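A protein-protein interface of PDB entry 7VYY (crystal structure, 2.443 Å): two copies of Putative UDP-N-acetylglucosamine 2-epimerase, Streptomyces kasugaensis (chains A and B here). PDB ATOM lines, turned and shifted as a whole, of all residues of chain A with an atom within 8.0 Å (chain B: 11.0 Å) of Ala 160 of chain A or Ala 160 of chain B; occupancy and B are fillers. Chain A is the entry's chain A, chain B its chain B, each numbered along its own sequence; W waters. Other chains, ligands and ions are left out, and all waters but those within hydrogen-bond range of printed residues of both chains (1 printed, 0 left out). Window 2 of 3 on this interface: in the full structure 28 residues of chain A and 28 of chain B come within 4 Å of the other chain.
Gln 142 of chain B touches Gln 142 of chain A.
Ala 160 of chain A touches Glu 161 of chain B.
Glu 161 of chain A touches Ala 160 of chain B.
O of Glu 161 of chain A touches CG of Glu 161 of chain B, 3.7 Å away.
The guanidinium group (NH2) of Arg 123 of chain B is in salt-bridge range of the side-chain carboxylate (OE1) of Glu 161 of chain B (2.8 Å).
NE2 of Gln 142 of chain A sits at hydrogen-bond distance from O of Glu 161 of chain A, at 3.1 Å.
The guanidinium group of Arg 123 of chain A is in salt-bridge range of the side-chain carboxylate of Glu 161 of chain A (2.8 Å).
O of Glu 161 of chain B lies within hydrogen-bond range of NE2 of Gln 142 of chain B (3.1 Å).
The backbone carbonyl oxygen (O) of Ala 160 of chain A lies within hydrogen-bond range of the backbone NH (N) of Gly 162 of chain B (3.4 Å).
O of Gln 142 of chain A lies within hydrogen-bond range of NH1 of Arg 138 of chain B, 2.8 Å away.
O of Ala 160 of chain B lies close to O of Ala 160 of chain A (3.0 Å).
The backbone NH (N) of Gly 162 of chain A is in hydrogen-bond range of the backbone carbonyl oxygen (O) of Ala 160 of chain B, at 3.5 Å.
Gln 142 of chain B touches its own counterpart, Gln 142 of chain A.
Ala 160 of chain A touches its own counterpart, Ala 160 of chain B.
Ala 160 of chain A touches Gly 162 of chain B, and with the chains exchanged Gly 162 of chain A touches Ala 160 of chain B.
Glu 161 of chain B touches its own counterpart, Glu 161 of chain A.
13 positions are printed for both chains.
Water W1 lies within hydrogen-bond range of the backbone carbonyl oxygen (O) of Gln 142 of chain A (2.8 Å) and the guanidinium group (NH2) of Arg 138 of chain B (3.2 Å).
Ala 160 of chain A touches three residues of chain B.
Ala 160 of chain B touches just these residues of chain A: Ala 160 (3.0 Å), Glu 161 (3.8 Å) and Gly 162 (3.5 Å).
No residue of chain B comes within 4 Å of Leu 159 of chain A.
Printed residues of chain B within 4 Å of Glu 161 of chain A: Ala 160 (3.8 Å) and Glu 161 (3.7 Å).
Of the printed residues of chain A, Arg 138 of chain B touches Gln 142 (2.8 Å).
Printed residues of chain A within 4 Å of Gly 162 of chain B: Ala 160 (3.4 Å).
Of the printed residues of chain A, Glu 161 of chain B touches Ala 160 (3.7 Å) and Glu 161 (3.7 Å).
Of the printed residues of chain A, Gln 142 of chain B touches Gln 142 (3.9 Å).
Printed residues of chain B within 4 Å of Gln 142 of chain A: Arg 138 and Gln 142.
Leu 159 of chain B touches none of the printed residues of chain A.
Val 163 of chain B touches none of the printed residues of chain A.
The nearest residue of chain B that does not touch Ala 160 of chain A is Leu 159 of chain B (4.4 Å).
Of the 23 printed residues of chain B, 5 touch a printed residue of chain A.
Among the printed residues, 8 pairs touch across the chains.
Among the printed residues, no Asp or Glu carboxylate lies within 4 Å of a Lys or Arg side-chain nitrogen of the other chain.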
ATOM      1  N   ARG A 123      11.290   7.513 -19.630  1.00  0.00           N
ATOM      2  CA  ARG A 123      12.610   6.959 -19.212  1.00  0.00           C
ATOM      3  C   ARG A 123      12.545   6.539 -17.735  1.00  0.00           C
ATOM      4  O   ARG A 123      12.172   7.365 -16.901  1.00  0.00           O
ATOM      5  CB  ARG A 123      13.726   7.990 -19.414  1.00  0.00           C
ATOM      6  CG  ARG A 123      13.960   8.427 -20.854  1.00  0.00           C
ATOM      7  CD  ARG A 123      14.570   7.343 -21.720  1.00  0.00           C
ATOM      8  NE  ARG A 123      14.833   7.790 -23.084  1.00  0.00           N
ATOM      9  CZ  ARG A 123      13.939   7.836 -24.083  1.00  0.00           C
ATOM     10  NH1 ARG A 123      12.680   7.481 -23.895  1.00  0.00           N
ATOM     11  NH2 ARG A 123      14.312   8.247 -25.283  1.00  0.00           N
ATOM     12  N   THR A 141      13.892   6.775 -30.556  1.00  0.00           N
ATOM     13  CA  THR A 141      14.093   8.236 -30.360  1.00  0.00           C
ATOM     14  C   THR A 141      15.129   8.764 -31.364  1.00  0.00           C
ATOM     15  O   THR A 141      14.970   9.904 -31.822  1.00  0.00           O
ATOM     16  CB  THR A 141      14.450   8.548 -28.905  1.00  0.00           C
ATOM     17  OG1 THR A 141      13.267   8.344 -28.133  1.00  0.00           O
ATOM     18  CG2 THR A 141      14.938   9.963 -28.697  1.00  0.00           C
ATOM     19  N   GLN A 142      16.146   7.971 -31.708  1.00  0.00           N
ATOM     20  CA  GLN A 142      17.190   8.384 -32.685  1.00  0.00           C
ATOM     21  C   GLN A 142      16.646   8.274 -34.118  1.00  0.00           C
ATOM     22  O   GLN A 142      17.138   9.024 -34.988  1.00  0.00           O
ATOM     23  CB  GLN A 142      18.468   7.566 -32.493  1.00  0.00           C
ATOM     24  CG  GLN A 142      19.200   7.891 -31.194  1.00  0.00           C
ATOM     25  CD  GLN A 142      19.410   9.371 -30.981  1.00  0.00           C
ATOM     26  OE1 GLN A 142      19.753  10.101 -31.901  1.00  0.00           O
ATOM     27  NE2 GLN A 142      19.212   9.834 -29.757  1.00  0.00           N
ATOM     28  N   ALA A 154       8.520  13.975 -20.271  1.00  0.00           N
ATOM     29  CA  ALA A 154       8.901  13.097 -21.405  1.00  0.00           C
ATOM     30  C   ALA A 154       9.630  13.928 -22.466  1.00  0.00           C
ATOM     31  O   ALA A 154      10.701  13.494 -22.921  1.00  0.00           O
ATOM     32  CB  ALA A 154       7.681  12.416 -21.975  1.00  0.00           C
ATOM     33  N   ALA A 155       9.061  15.079 -22.834  1.00  0.00           N
ATOM     34  CA  ALA A 155       9.657  16.054 -23.785  1.00  0.00           C
ATOM     35  C   ALA A 155      11.079  16.403 -23.317  1.00  0.00           C
ATOM     36  O   ALA A 155      12.002  16.329 -24.142  1.00  0.00           O
ATOM     37  CB  ALA A 155       8.789  17.285 -23.900  1.00  0.00           C
ATOM     38  N   GLY A 156      11.245  16.713 -22.027  1.00  0.00           N
ATOM     39  CA  GLY A 156      12.552  17.008 -21.403  1.00  0.00           C
ATOM     40  C   GLY A 156      13.560  15.894 -21.647  1.00  0.00           C
ATOM     41  O   GLY A 156      14.731  16.206 -21.920  1.00  0.00           O
ATOM     42  N   ASN A 157      13.131  14.633 -21.558  1.00  0.00           N
ATOM     43  CA  ASN A 157      14.022  13.450 -21.695  1.00  0.00           C
ATOM     44  C   ASN A 157      14.553  13.345 -23.129  1.00  0.00           C
ATOM     45  O   ASN A 157      15.683  12.871 -23.297  1.00  0.00           O
ATOM     46  CB  ASN A 157      13.310  12.154 -21.317  1.00  0.00           C
ATOM     47  CG  ASN A 157      12.973  12.061 -19.844  1.00  0.00           C
ATOM     48  OD1 ASN A 157      13.648  12.646 -19.000  1.00  0.00           O
ATOM     49  ND2 ASN A 157      11.946  11.292 -19.523  1.00  0.00           N
ATOM     50  N   LEU A 158      13.740  13.732 -24.118  1.00  0.00           N
ATOM     51  CA  LEU A 158      14.111  13.689 -25.558  1.00  0.00           C
ATOM     52  C   LEU A 158      15.207  14.726 -25.843  1.00  0.00           C
ATOM     53  O   LEU A 158      16.112  14.410 -26.621  1.00  0.00           O
ATOM     54  CB  LEU A 158      12.864  13.932 -26.414  1.00  0.00           C
ATOM     55  CG  LEU A 158      11.798  12.841 -26.331  1.00  0.00           C
ATOM     56  CD1 LEU A 158      10.521  13.280 -27.027  1.00  0.00           C
ATOM     57  CD2 LEU A 158      12.304  11.524 -26.906  1.00  0.00           C
ATOM     58  N   LEU A 159      15.154  15.894 -25.197  1.00  0.00           N
ATOM     59  CA  LEU A 159      16.154  16.991 -25.359  1.00  0.00           C
ATOM     60  C   LEU A 159      17.530  16.536 -24.846  1.00  0.00           C
ATOM     61  O   LEU A 159      18.531  16.773 -25.544  1.00  0.00           O
ATOM     62  CB  LEU A 159      15.656  18.241 -24.634  1.00  0.00           C
ATOM     63  CG  LEU A 159      14.339  18.823 -25.156  1.00  0.00           C
ATOM     64  CD1 LEU A 159      13.921  20.061 -24.367  1.00  0.00           C
ATOM     65  CD2 LEU A 159      14.418  19.156 -26.636  1.00  0.00           C
ATOM     66  N   ALA A 160      17.567  15.834 -23.711  1.00  0.00           N
ATOM     67  CA  ALA A 160      18.794  15.269 -23.096  1.00  0.00           C
ATOM     68  C   ALA A 160      19.455  14.244 -24.024  1.00  0.00           C
ATOM     69  O   ALA A 160      20.658  13.974 -23.829  1.00  0.00           O
ATOM     70  CB  ALA A 160      18.458  14.649 -21.762  1.00  0.00           C
ATOM     71  N   GLU A 161      18.714  13.678 -24.981  1.00  0.00           N
ATOM     72  CA  GLU A 161      19.242  12.667 -25.942  1.00  0.00           C
ATOM     73  C   GLU A 161      19.485  13.298 -27.325  1.00  0.00           C
ATOM     74  O   GLU A 161      19.754  12.536 -28.274  1.00  0.00           O
ATOM     75  CB  GLU A 161      18.312  11.454 -25.969  1.00  0.00           C
ATOM     76  CG  GLU A 161      18.549  10.541 -24.782  1.00  0.00           C
ATOM     77  CD  GLU A 161      17.534   9.439 -24.552  1.00  0.00           C
ATOM     78  OE1 GLU A 161      16.980   8.919 -25.545  1.00  0.00           O
ATOM     79  OE2 GLU A 161      17.307   9.098 -23.373  1.00  0.00           O
ATOM     80  N   GLY A 162      19.452  14.631 -27.426  1.00  0.00           N
ATOM     81  CA  GLY A 162      19.914  15.383 -28.615  1.00  0.00           C
ATOM     82  C   GLY A 162      18.798  15.699 -29.599  1.00  0.00           C
ATOM     83  O   GLY A 162      19.097  16.212 -30.688  1.00  0.00           O
ATOM     84  N   VAL A 163      17.545  15.428 -29.244  1.00  0.00           N
ATOM     85  CA  VAL A 163      16.378  15.727 -30.122  1.00  0.00           C
ATOM     86  C   VAL A 163      16.163  17.249 -30.125  1.00  0.00           C
ATOM     87  O   VAL A 163      16.238  17.867 -29.050  1.00  0.00           O
ATOM     88  CB  VAL A 163      15.119  14.963 -29.671  1.00  0.00           C
ATOM     89  CG1 VAL A 163      13.906  15.312 -30.522  1.00  0.00           C
ATOM     90  CG2 VAL A 163      15.352  13.462 -29.670  1.00  0.00           C
ATOM     91  N   GLY B 121      31.576   9.010 -31.425  1.00  0.00           N
ATOM     92  CA  GLY B 121      31.265  10.407 -31.067  1.00  0.00           C
ATOM     93  C   GLY B 121      31.440  11.398 -32.212  1.00  0.00           C
ATOM     94  O   GLY B 121      31.157  12.596 -31.983  1.00  0.00           O
ATOM     95  N   LEU B 122      31.884  10.970 -33.393  1.00  0.00           N
ATOM     96  CA  LEU B 122      31.987  11.866 -34.580  1.00  0.00           C
ATOM     97  C   LEU B 122      30.583  12.267 -35.043  1.00  0.00           C
ATOM     98  O   LEU B 122      29.754  11.373 -35.250  1.00  0.00           O
ATOM     99  CB  LEU B 122      32.770  11.170 -35.695  1.00  0.00           C
ATOM    100  CG  LEU B 122      34.237  10.892 -35.365  1.00  0.00           C
ATOM    101  CD1 LEU B 122      34.939  10.223 -36.532  1.00  0.00           C
ATOM    102  CD2 LEU B 122      34.962  12.169 -34.964  1.00  0.00           C
ATOM    103  N   ARG B 123      30.328  13.570 -35.168  1.00  0.00           N
ATOM    104  CA  ARG B 123      29.016  14.131 -35.595  1.00  0.00           C
ATOM    105  C   ARG B 123      29.271  15.263 -36.601  1.00  0.00           C
ATOM    106  O   ARG B 123      30.006  16.201 -36.255  1.00  0.00           O
ATOM    107  CB  ARG B 123      28.221  14.653 -34.389  1.00  0.00           C
ATOM    108  CG  ARG B 123      27.863  13.604 -33.342  1.00  0.00           C
ATOM    109  CD  ARG B 123      26.807  12.617 -33.806  1.00  0.00           C
ATOM    110  NE  ARG B 123      26.412  11.658 -32.778  1.00  0.00           N
ATOM    111  CZ  ARG B 123      27.074  10.537 -32.461  1.00  0.00           C
ATOM    112  NH1 ARG B 123      28.199  10.206 -33.078  1.00  0.00           N
ATOM    113  NH2 ARG B 123      26.596   9.738 -31.519  1.00  0.00           N
ATOM    114  N   GLY B 125      26.728  17.064 -37.650  1.00  0.00           N
ATOM    115  CA  GLY B 125      25.638  17.994 -37.292  1.00  0.00           C
ATOM    116  C   GLY B 125      24.685  18.197 -38.459  1.00  0.00           C
ATOM    117  O   GLY B 125      24.012  19.252 -38.497  1.00  0.00           O
ATOM    118  N   ARG B 138      24.377   7.267 -34.240  1.00  0.00           N
ATOM    119  CA  ARG B 138      23.490   7.619 -33.099  1.00  0.00           C
ATOM    120  C   ARG B 138      22.850   6.337 -32.554  1.00  0.00           C
ATOM    121  O   ARG B 138      22.680   6.234 -31.332  1.00  0.00           O
ATOM    122  CB  ARG B 138      22.495   8.703 -33.525  1.00  0.00           C
ATOM    123  CG  ARG B 138      23.157  10.059 -33.732  1.00  0.00           C
ATOM    124  CD  ARG B 138      22.180  11.210 -33.908  1.00  0.00           C
ATOM    125  NE  ARG B 138      21.615  11.222 -35.251  1.00  0.00           N
ATOM    126  CZ  ARG B 138      20.393  10.817 -35.582  1.00  0.00           C
ATOM    127  NH1 ARG B 138      19.541  10.389 -34.664  1.00  0.00           N
ATOM    128  NH2 ARG B 138      20.009  10.879 -36.846  1.00  0.00           N
ATOM    129  N   THR B 141      25.584   4.379 -30.635  1.00  0.00           N
ATOM    130  CA  THR B 141      25.842   5.152 -29.390  1.00  0.00           C
ATOM    131  C   THR B 141      24.835   4.749 -28.303  1.00  0.00           C
ATOM    132  O   THR B 141      25.242   4.718 -27.125  1.00  0.00           O
ATOM    133  CB  THR B 141      25.859   6.657 -29.674  1.00  0.00           C
ATOM    134  OG1 THR B 141      27.059   6.917 -30.405  1.00  0.00           O
ATOM    135  CG2 THR B 141      25.821   7.514 -28.430  1.00  0.00           C
ATOM    136  N   GLN B 142      23.585   4.444 -28.663  1.00  0.00           N
ATOM    137  CA  GLN B 142      22.542   4.048 -27.674  1.00  0.00           C
ATOM    138  C   GLN B 142      22.761   2.590 -27.247  1.00  0.00           C
ATOM    139  O   GLN B 142      22.383   2.265 -26.101  1.00  0.00           O
ATOM    140  CB  GLN B 142      21.134   4.270 -28.224  1.00  0.00           C
ATOM    141  CG  GLN B 142      20.767   5.738 -28.385  1.00  0.00           C
ATOM    142  CD  GLN B 142      21.057   6.564 -27.156  1.00  0.00           C
ATOM    143  OE1 GLN B 142      20.800   6.141 -26.032  1.00  0.00           O
ATOM    144  NE2 GLN B 142      21.578   7.766 -27.359  1.00  0.00           N
ATOM    145  N   HIS B 147      32.453   3.361 -24.884  1.00  0.00           N
ATOM    146  CA  HIS B 147      32.685   4.262 -26.049  1.00  0.00           C
ATOM    147  C   HIS B 147      34.156   4.655 -26.127  1.00  0.00           C
ATOM    148  O   HIS B 147      34.616   5.355 -25.210  1.00  0.00           O
ATOM    149  CB  HIS B 147      31.816   5.520 -25.955  1.00  0.00           C
ATOM    150  CG  HIS B 147      30.372   5.220 -25.760  1.00  0.00           C
ATOM    151  ND1 HIS B 147      29.499   5.097 -26.822  1.00  0.00           N
ATOM    152  CD2 HIS B 147      29.650   5.011 -24.638  1.00  0.00           C
ATOM    153  CE1 HIS B 147      28.297   4.828 -26.363  1.00  0.00           C
ATOM    154  NE2 HIS B 147      28.360   4.764 -25.021  1.00  0.00           N
ATOM    155  N   ALA B 152      38.550  14.593 -27.558  1.00  0.00           N
ATOM    156  CA  ALA B 152      37.764  15.222 -26.470  1.00  0.00           C
ATOM    157  C   ALA B 152      36.416  15.697 -27.023  1.00  0.00           C
ATOM    158  O   ALA B 152      35.406  15.533 -26.323  1.00  0.00           O
ATOM    159  CB  ALA B 152      38.539  16.360 -25.847  1.00  0.00           C
ATOM    160  N   ASP B 153      36.417  16.265 -28.233  1.00  0.00           N
ATOM    161  CA  ASP B 153      35.208  16.804 -28.920  1.00  0.00           C
ATOM    162  C   ASP B 153      34.196  15.672 -29.164  1.00  0.00           C
ATOM    163  O   ASP B 153      32.989  15.886 -28.908  1.00  0.00           O
ATOM    164  CB  ASP B 153      35.591  17.509 -30.222  1.00  0.00           C
ATOM    165  CG  ASP B 153      34.398  18.049 -30.980  1.00  0.00           C
ATOM    166  OD1 ASP B 153      33.780  19.020 -30.488  1.00  0.00           O
ATOM    167  OD2 ASP B 153      34.081  17.477 -32.037  1.00  0.00           O
ATOM    168  N   ALA B 154      34.665  14.518 -29.646  1.00  0.00           N
ATOM    169  CA  ALA B 154      33.843  13.307 -29.878  1.00  0.00           C
ATOM    170  C   ALA B 154      33.184  12.870 -28.564  1.00  0.00           C
ATOM    171  O   ALA B 154      31.961  12.633 -28.567  1.00  0.00           O
ATOM    172  CB  ALA B 154      34.687  12.205 -30.469  1.00  0.00           C
ATOM    173  N   ALA B 155      33.970  12.782 -27.485  1.00  0.00           N
ATOM    174  CA  ALA B 155      33.500  12.461 -26.114  1.00  0.00           C
ATOM    175  C   ALA B 155      32.367  13.421 -25.733  1.00  0.00           C
ATOM    176  O   ALA B 155      31.318  12.942 -25.269  1.00  0.00           O
ATOM    177  CB  ALA B 155      34.645  12.525 -25.129  1.00  0.00           C
ATOM    178  N   GLY B 156      32.562  14.722 -25.956  1.00  0.00           N
ATOM    179  CA  GLY B 156      31.544  15.766 -25.721  1.00  0.00           C
ATOM    180  C   GLY B 156      30.230  15.460 -26.430  1.00  0.00           C
ATOM    181  O   GLY B 156      29.167  15.685 -25.820  1.00  0.00           O
ATOM    182  N   ASN B 157      30.288  14.954 -27.667  1.00  0.00           N
ATOM    183  CA  ASN B 157      29.088  14.680 -28.505  1.00  0.00           C
ATOM    184  C   ASN B 157      28.278  13.531 -27.905  1.00  0.00           C
ATOM    185  O   ASN B 157      27.037  13.552 -28.056  1.00  0.00           O
ATOM    186  CB  ASN B 157      29.447  14.330 -29.952  1.00  0.00           C
ATOM    187  CG  ASN B 157      30.021  15.503 -30.714  1.00  0.00           C
ATOM    188  OD1 ASN B 157      29.725  16.652 -30.412  1.00  0.00           O
ATOM    189  ND2 ASN B 157      30.829  15.213 -31.717  1.00  0.00           N
ATOM    190  N   LEU B 158      28.954  12.563 -27.280  1.00  0.00           N
ATOM    191  CA  LEU B 158      28.302  11.380 -26.654  1.00  0.00           C
ATOM    192  C   LEU B 158      27.498  11.829 -25.427  1.00  0.00           C
ATOM    193  O   LEU B 158      26.391  11.295 -25.228  1.00  0.00           O
ATOM    194  CB  LEU B 158      29.366  10.332 -26.306  1.00  0.00           C
ATOM    195  CG  LEU B 158      30.089   9.719 -27.507  1.00  0.00           C
ATOM    196  CD1 LEU B 158      31.277   8.876 -27.064  1.00  0.00           C
ATOM    197  CD2 LEU B 158      29.136   8.893 -28.361  1.00  0.00           C
ATOM    198  N   LEU B 159      28.010  12.799 -24.665  1.00  0.00           N
ATOM    199  CA  LEU B 159      27.345  13.340 -23.442  1.00  0.00           C
ATOM    200  C   LEU B 159      26.036  14.048 -23.827  1.00  0.00           C
ATOM    201  O   LEU B 159      25.033  13.844 -23.129  1.00  0.00           O
ATOM    202  CB  LEU B 159      28.310  14.287 -22.716  1.00  0.00           C
ATOM    203  CG  LEU B 159      29.229  13.636 -21.679  1.00  0.00           C
ATOM    204  CD1 LEU B 159      29.922  12.395 -22.230  1.00  0.00           C
ATOM    205  CD2 LEU B 159      30.249  14.643 -21.177  1.00  0.00           C
ATOM    206  N   ALA B 160      26.036  14.811 -24.922  1.00  0.00           N
ATOM    207  CA  ALA B 160      24.858  15.540 -25.458  1.00  0.00           C
ATOM    208  C   ALA B 160      23.740  14.561 -25.846  1.00  0.00           C
ATOM    209  O   ALA B 160      22.570  15.005 -25.918  1.00  0.00           O
ATOM    210  CB  ALA B 160      25.265  16.379 -26.642  1.00  0.00           C
ATOM    211  N   GLU B 161      24.071  13.286 -26.088  1.00  0.00           N
ATOM    212  CA  GLU B 161      23.084  12.237 -26.468  1.00  0.00           C
ATOM    213  C   GLU B 161      22.772  11.307 -25.282  1.00  0.00           C
ATOM    214  O   GLU B 161      22.169  10.233 -25.519  1.00  0.00           O
ATOM    215  CB  GLU B 161      23.596  11.505 -27.705  1.00  0.00           C
ATOM    216  CG  GLU B 161      23.339  12.300 -28.976  1.00  0.00           C
ATOM    217  CD  GLU B 161      24.051  11.800 -30.217  1.00  0.00           C
ATOM    218  OE1 GLU B 161      24.238  10.568 -30.323  1.00  0.00           O
ATOM    219  OE2 GLU B 161      24.418  12.651 -31.074  1.00  0.00           O
ATOM    220  N   GLY B 162      23.143  11.710 -24.059  1.00  0.00           N
ATOM    221  CA  GLY B 162      22.710  11.075 -22.794  1.00  0.00           C
ATOM    222  C   GLY B 162      23.639   9.966 -22.319  1.00  0.00           C
ATOM    223  O   GLY B 162      23.256   9.238 -21.394  1.00  0.00           O
ATOM    224  N   VAL B 163      24.823   9.828 -22.912  1.00  0.00           N
ATOM    225  CA  VAL B 163      25.822   8.810 -22.472  1.00  0.00           C
ATOM    226  C   VAL B 163      26.416   9.262 -21.131  1.00  0.00           C
ATOM    227  O   VAL B 163      26.710  10.463 -20.984  1.00  0.00           O
ATOM    228  CB  VAL B 163      26.895   8.562 -23.547  1.00  0.00           C
ATOM    229  CG1 VAL B 163      27.958   7.579 -23.088  1.00  0.00           C
ATOM    230  CG2 VAL B 163      26.265   8.050 -24.832  1.00  0.00           C
ATOM    231  N   ARG B 164      26.559   8.327 -20.188  1.00  0.00           N
ATOM    232  CA  ARG B 164      27.241   8.533 -18.878  1.00  0.00           C
ATOM    233  C   ARG B 164      28.747   8.710 -19.101  1.00  0.00           C
ATOM    234  O   ARG B 164      29.333   7.928 -19.886  1.00  0.00           O
ATOM    235  CB  ARG B 164      27.009   7.333 -17.954  1.00  0.00           C
ATOM    236  CG  ARG B 164      25.556   7.123 -17.555  1.00  0.00           C
ATOM    237  CD  ARG B 164      25.256   5.679 -17.207  1.00  0.00           C
ATOM    238  NE  ARG B 164      26.212   5.124 -16.252  1.00  0.00           N
ATOM    239  CZ  ARG B 164      26.629   3.851 -16.224  1.00  0.00           C
ATOM    240  NH1 ARG B 164      26.206   2.979 -17.124  1.00  0.00           N
ATOM    241  NH2 ARG B 164      27.485   3.457 -15.296  1.00  0.00           N
ATOM    242  N   SER B 165      29.347   9.678 -18.402  1.00  0.00           N
ATOM    243  CA  SER B 165      30.790  10.033 -18.497  1.00  0.00           C
ATOM    244  C   SER B 165      31.666   8.803 -18.223  1.00  0.00           C
ATOM    245  O   SER B 165      32.725   8.678 -18.880  1.00  0.00           O
ATOM    246  CB  SER B 165      31.105  11.161 -17.563  1.00  0.00           C
ATOM    247  OG  SER B 165      30.007  12.063 -17.504  1.00  0.00           O
ATOM    248  N   VAL B 168      32.587   6.663 -21.305  1.00  0.00           N
ATOM    249  CA  VAL B 168      33.336   7.330 -22.413  1.00  0.00           C
ATOM    250  C   VAL B 168      34.827   7.429 -22.058  1.00  0.00           C
ATOM    251  O   VAL B 168      35.161   8.048 -21.036  1.00  0.00           O
ATOM    252  CB  VAL B 168      32.741   8.709 -22.749  1.00  0.00           C
ATOM    253  CG1 VAL B 168      33.536   9.400 -23.840  1.00  0.00           C
ATOM    254  CG2 VAL B 168      31.279   8.609 -23.146  1.00  0.00           C
HETATM  255  O   HOH W   1      16.977  10.079 -37.573  1.00  0.00           O
